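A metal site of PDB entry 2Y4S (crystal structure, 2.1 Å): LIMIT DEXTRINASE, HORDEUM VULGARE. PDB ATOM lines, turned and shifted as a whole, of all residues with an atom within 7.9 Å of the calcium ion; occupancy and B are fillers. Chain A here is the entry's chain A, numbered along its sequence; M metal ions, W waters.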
ATOM      1  N   GLY A 313      16.931  25.475   9.198  1.00  0.00           N
ATOM      2  CA  GLY A 313      16.621  25.356  10.616  1.00  0.00           C
ATOM      3  C   GLY A 313      15.348  26.064  11.011  1.00  0.00           C
ATOM      4  O   GLY A 313      14.836  25.868  12.109  1.00  0.00           O
ATOM      5  N   VAL A 314      14.835  26.890  10.111  1.00  0.00           N
ATOM      6  CA  VAL A 314      13.566  27.595  10.321  1.00  0.00           C
ATOM      7  C   VAL A 314      12.753  27.571   9.033  1.00  0.00           C
ATOM      8  O   VAL A 314      13.248  27.946   7.964  1.00  0.00           O
ATOM      9  CB  VAL A 314      13.787  29.072  10.725  1.00  0.00           C
ATOM     10  CG1 VAL A 314      12.450  29.782  10.856  1.00  0.00           C
ATOM     11  CG2 VAL A 314      14.577  29.165  12.034  1.00  0.00           C
ATOM     12  N   ASP A 315      11.510  27.111   9.121  1.00  0.00           N
ATOM     13  CA  ASP A 315      10.623  27.078   7.963  1.00  0.00           C
ATOM     14  C   ASP A 315      10.239  28.502   7.578  1.00  0.00           C
ATOM     15  O   ASP A 315       9.854  29.306   8.446  1.00  0.00           O
ATOM     16  CB  ASP A 315       9.382  26.247   8.297  1.00  0.00           C
ATOM     17  CG  ASP A 315       8.630  25.782   7.067  1.00  0.00           C
ATOM     18  OD1 ASP A 315       8.548  26.539   6.085  1.00  0.00           O
ATOM     19  OD2 ASP A 315       8.112  24.639   7.089  1.00  0.00           O
ATOM     20  N   VAL A 343      10.185  23.843  25.353  1.00  0.00           N
ATOM     21  CA  VAL A 343      10.881  24.429  24.206  1.00  0.00           C
ATOM     22  C   VAL A 343      11.542  23.349  23.353  1.00  0.00           C
ATOM     23  O   VAL A 343      11.372  23.315  22.131  1.00  0.00           O
ATOM     24  CB  VAL A 343      11.938  25.457  24.657  1.00  0.00           C
ATOM     25  CG1 VAL A 343      12.726  25.973  23.453  1.00  0.00           C
ATOM     26  CG2 VAL A 343      11.273  26.609  25.394  1.00  0.00           C
ATOM     27  N   ILE A 346       9.543  21.362  20.756  1.00  0.00           N
ATOM     28  CA  ILE A 346       9.133  21.957  19.480  1.00  0.00           C
ATOM     29  C   ILE A 346      10.254  22.697  18.764  1.00  0.00           C
ATOM     30  O   ILE A 346      10.044  23.288  17.705  1.00  0.00           O
ATOM     31  CB  ILE A 346       7.959  22.958  19.668  1.00  0.00           C
ATOM     32  CG1 ILE A 346       8.416  24.158  20.494  1.00  0.00           C
ATOM     33  CG2 ILE A 346       6.752  22.274  20.302  1.00  0.00           C
ATOM     34  CD1 ILE A 346       7.469  25.328  20.451  1.00  0.00           C
ATOM     35  N   GLN A 347      11.451  22.673  19.346  1.00  0.00           N
ATOM     36  CA  GLN A 347      12.541  23.502  18.860  1.00  0.00           C
ATOM     37  C   GLN A 347      12.921  23.248  17.401  1.00  0.00           C
ATOM     38  O   GLN A 347      13.535  24.086  16.781  1.00  0.00           O
ATOM     39  CB  GLN A 347      13.782  23.383  19.757  1.00  0.00           C
ATOM     40  CG  GLN A 347      14.566  22.093  19.545  1.00  0.00           C
ATOM     41  CD  GLN A 347      15.695  21.933  20.551  1.00  0.00           C
ATOM     42  OE1 GLN A 347      16.173  22.905  21.134  1.00  0.00           O
ATOM     43  NE2 GLN A 347      16.142  20.701  20.733  1.00  0.00           N
ATOM     44  N   GLU A 348      12.572  22.090  16.866  1.00  0.00           N
ATOM     45  CA  GLU A 348      12.937  21.796  15.484  1.00  0.00           C
ATOM     46  C   GLU A 348      11.953  22.401  14.481  1.00  0.00           C
ATOM     47  O   GLU A 348      12.224  22.451  13.281  1.00  0.00           O
ATOM     48  CB  GLU A 348      13.082  20.291  15.244  1.00  0.00           C
ATOM     49  CG  GLU A 348      14.236  19.660  16.011  1.00  0.00           C
ATOM     50  CD  GLU A 348      15.577  20.266  15.647  1.00  0.00           C
ATOM     51  OE1 GLU A 348      15.838  20.454  14.445  1.00  0.00           O
ATOM     52  OE2 GLU A 348      16.378  20.543  16.560  1.00  0.00           O
ATOM     53  N   GLU A 349      10.808  22.854  14.974  1.00  0.00           N
ATOM     54  CA  GLU A 349       9.762  23.387  14.099  1.00  0.00           C
ATOM     55  C   GLU A 349       9.221  24.734  14.554  1.00  0.00           C
ATOM     56  O   GLU A 349       8.137  25.134  14.145  1.00  0.00           O
ATOM     57  CB  GLU A 349       8.609  22.380  13.977  1.00  0.00           C
ATOM     58  CG  GLU A 349       8.995  21.026  13.410  1.00  0.00           C
ATOM     59  CD  GLU A 349       9.283  20.007  14.495  1.00  0.00           C
ATOM     60  OE1 GLU A 349       8.627  20.072  15.564  1.00  0.00           O
ATOM     61  OE2 GLU A 349      10.143  19.128  14.285  1.00  0.00           O
ATOM     62  N   ASP A 350       9.968  25.429  15.415  1.00  0.00           N
ATOM     63  CA  ASP A 350       9.545  26.761  15.854  1.00  0.00           C
ATOM     64  C   ASP A 350      10.152  27.825  14.942  1.00  0.00           C
ATOM     65  O   ASP A 350      10.830  27.498  13.969  1.00  0.00           O
ATOM     66  CB  ASP A 350       9.866  26.979  17.333  1.00  0.00           C
ATOM     67  CG  ASP A 350      11.339  27.195  17.592  1.00  0.00           C
ATOM     68  OD1 ASP A 350      12.104  27.245  16.611  1.00  0.00           O
ATOM     69  OD2 ASP A 350      11.722  27.332  18.767  1.00  0.00           O
ATOM     70  N   PRO A 351       9.908  29.121  15.240  1.00  0.00           N
ATOM     71  CA  PRO A 351      10.393  30.135  14.304  1.00  0.00           C
ATOM     72  C   PRO A 351      11.846  30.558  14.546  1.00  0.00           C
ATOM     73  O   PRO A 351      12.301  31.494  13.887  1.00  0.00           O
ATOM     74  CB  PRO A 351       9.483  31.342  14.604  1.00  0.00           C
ATOM     75  CG  PRO A 351       8.441  30.862  15.596  1.00  0.00           C
ATOM     76  CD  PRO A 351       9.071  29.705  16.296  1.00  0.00           C
ATOM     77  N   TYR A 352      12.549  29.884  15.446  1.00  0.00           N
ATOM     78  CA  TYR A 352      13.786  30.436  15.991  1.00  0.00           C
ATOM     79  C   TYR A 352      15.083  29.707  15.640  1.00  0.00           C
ATOM     80  O   TYR A 352      15.168  28.494  15.740  1.00  0.00           O
ATOM     81  CB  TYR A 352      13.690  30.526  17.510  1.00  0.00           C
ATOM     82  CG  TYR A 352      14.768  31.408  18.097  1.00  0.00           C
ATOM     83  CD1 TYR A 352      16.028  30.903  18.378  1.00  0.00           C
ATOM     84  CD2 TYR A 352      14.521  32.755  18.332  1.00  0.00           C
ATOM     85  CE1 TYR A 352      17.018  31.726  18.904  1.00  0.00           C
ATOM     86  CE2 TYR A 352      15.506  33.577  18.845  1.00  0.00           C
ATOM     87  CZ  TYR A 352      16.751  33.059  19.133  1.00  0.00           C
ATOM     88  OH  TYR A 352      17.714  33.891  19.647  1.00  0.00           O
ATOM     89  N   ASN A 353      16.106  30.464  15.269  1.00  0.00           N
ATOM     90  CA  ASN A 353      17.453  29.928  15.126  1.00  0.00           C
ATOM     91  C   ASN A 353      18.434  31.067  14.907  1.00  0.00           C
ATOM     92  O   ASN A 353      18.094  32.037  14.235  1.00  0.00           O
ATOM     93  CB  ASN A 353      17.526  28.917  13.975  1.00  0.00           C
ATOM     94  CG  ASN A 353      18.756  28.023  14.057  1.00  0.00           C
ATOM     95  OD1 ASN A 353      19.890  28.472  13.832  1.00  0.00           O
ATOM     96  ND2 ASN A 353      18.543  26.752  14.381  1.00  0.00           N
ATOM     97  N   TRP A 354      19.633  30.967  15.469  1.00  0.00           N
ATOM     98  CA  TRP A 354      20.625  32.013  15.219  1.00  0.00           C
ATOM     99  C   TRP A 354      20.829  32.163  13.721  1.00  0.00           C
ATOM    100  O   TRP A 354      20.962  33.275  13.223  1.00  0.00           O
ATOM    101  CB  TRP A 354      21.959  31.706  15.896  1.00  0.00           C
ATOM    102  CG  TRP A 354      21.992  31.978  17.369  1.00  0.00           C
ATOM    103  CD1 TRP A 354      21.095  32.714  18.090  1.00  0.00           C
ATOM    104  CD2 TRP A 354      22.994  31.553  18.294  1.00  0.00           C
ATOM    105  NE1 TRP A 354      21.473  32.754  19.410  1.00  0.00           N
ATOM    106  CE2 TRP A 354      22.628  32.047  19.567  1.00  0.00           C
ATOM    107  CE3 TRP A 354      24.155  30.778  18.177  1.00  0.00           C
ATOM    108  CZ2 TRP A 354      23.389  31.799  20.706  1.00  0.00           C
ATOM    109  CZ3 TRP A 354      24.909  30.535  19.311  1.00  0.00           C
ATOM    110  CH2 TRP A 354      24.524  31.039  20.561  1.00  0.00           C
ATOM    111  N   TYR A 699      21.372  28.982  20.627  1.00  0.00           N
ATOM    112  CA  TYR A 699      21.104  29.012  19.190  1.00  0.00           C
ATOM    113  C   TYR A 699      19.757  28.409  18.799  1.00  0.00           C
ATOM    114  O   TYR A 699      19.172  28.776  17.782  1.00  0.00           O
ATOM    115  CB  TYR A 699      22.227  28.286  18.429  1.00  0.00           C
ATOM    116  CG  TYR A 699      22.132  26.775  18.486  1.00  0.00           C
ATOM    117  CD1 TYR A 699      22.505  26.070  19.622  1.00  0.00           C
ATOM    118  CD2 TYR A 699      21.662  26.043  17.391  1.00  0.00           C
ATOM    119  CE1 TYR A 699      22.409  24.686  19.674  1.00  0.00           C
ATOM    120  CE2 TYR A 699      21.582  24.666  17.429  1.00  0.00           C
ATOM    121  CZ  TYR A 699      21.950  23.990  18.580  1.00  0.00           C
ATOM    122  OH  TYR A 699      21.861  22.624  18.621  1.00  0.00           O
ATOM    123  N   ASN A 700      19.276  27.468  19.607  1.00  0.00           N
ATOM    124  CA  ASN A 700      18.049  26.736  19.295  1.00  0.00           C
ATOM    125  C   ASN A 700      17.088  26.769  20.467  1.00  0.00           C
ATOM    126  O   ASN A 700      16.206  25.913  20.586  1.00  0.00           O
ATOM    127  CB  ASN A 700      18.393  25.289  18.926  1.00  0.00           C
ATOM    128  CG  ASN A 700      17.379  24.666  17.987  1.00  0.00           C
ATOM    129  OD1 ASN A 700      16.595  25.362  17.356  1.00  0.00           O
ATOM    130  ND2 ASN A 700      17.394  23.339  17.868  1.00  0.00           N
ATOM    131  N   SER A 701      17.268  27.753  21.348  1.00  0.00           N
ATOM    132  CA  SER A 701      16.528  27.832  22.603  1.00  0.00           C
ATOM    133  C   SER A 701      15.241  28.657  22.509  1.00  0.00           C
ATOM    134  O   SER A 701      14.623  28.961  23.536  1.00  0.00           O
ATOM    135  CB  SER A 701      17.425  28.375  23.717  1.00  0.00           C
ATOM    136  OG  SER A 701      18.496  27.479  23.971  1.00  0.00           O
ATOM    137  N   GLY A 702      14.856  29.012  21.288  1.00  0.00           N
ATOM    138  CA  GLY A 702      13.573  29.662  21.048  1.00  0.00           C
ATOM    139  C   GLY A 702      13.456  31.065  21.618  1.00  0.00           C
ATOM    140  O   GLY A 702      14.388  31.600  22.205  1.00  0.00           O
ATOM    141  N   ASP A 703      12.290  31.671  21.431  1.00  0.00           N
ATOM    142  CA  ASP A 703      12.035  33.011  21.945  1.00  0.00           C
ATOM    143  C   ASP A 703      12.057  33.046  23.464  1.00  0.00           C
ATOM    144  O   ASP A 703      12.343  34.085  24.062  1.00  0.00           O
ATOM    145  CB  ASP A 703      10.691  33.541  21.430  1.00  0.00           C
ATOM    146  CG  ASP A 703      10.704  33.821  19.950  1.00  0.00           C
ATOM    147  OD1 ASP A 703      11.756  34.248  19.438  1.00  0.00           O
ATOM    148  OD2 ASP A 703       9.661  33.618  19.301  1.00  0.00           O
HETATM  149 CA    CA M   1      14.468  26.270  16.279  1.00  0.00          CA
HETATM  150  O   HOH W   1      14.329  27.142  18.910  1.00  0.00           O
HETATM  151  O   HOH W   2      16.069  25.361  14.352  1.00  0.00           O
HETATM  152  O   HOH W   3      12.982  26.172  13.978  1.00  0.00           O
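The calcium ion is bound by the backbone carbonyl oxygen of Tyr 352 (2.4 Å), the backbone carbonyl oxygen of Gln 347 (2.4 Å), the side-chain amide oxygen of Asn 700 (2.6 Å), the side-chain carboxylate of Asp 350 (2.6 Å), water W2 (2.7 Å), water W3 (2.7 Å) and water W1 (2.8 Å).
Along chain A the residues within 4 Å of the calcium ion span positions 347 to 700.
The side-chain amide nitrogen (ND2) of Asn 700 lies within hydrogen-bond range of the side-chain carboxylate (OE2) of Glu 348, at 3.2 Å.
Water W2 lies within hydrogen-bond range of O of Gly 313 (2.6 Å) and ND2 of Asn 353 (2.8 Å). Water W1 lies within hydrogen-bond range of the side-chain carboxylate of Asp 350 (2.6 Å), the backbone carbonyl oxygen of Asn 700 (2.8 Å) and the backbone NH of Gly 702 (3.1 Å). Water W3 bridges O of Asp 350 and O of Gly 313.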
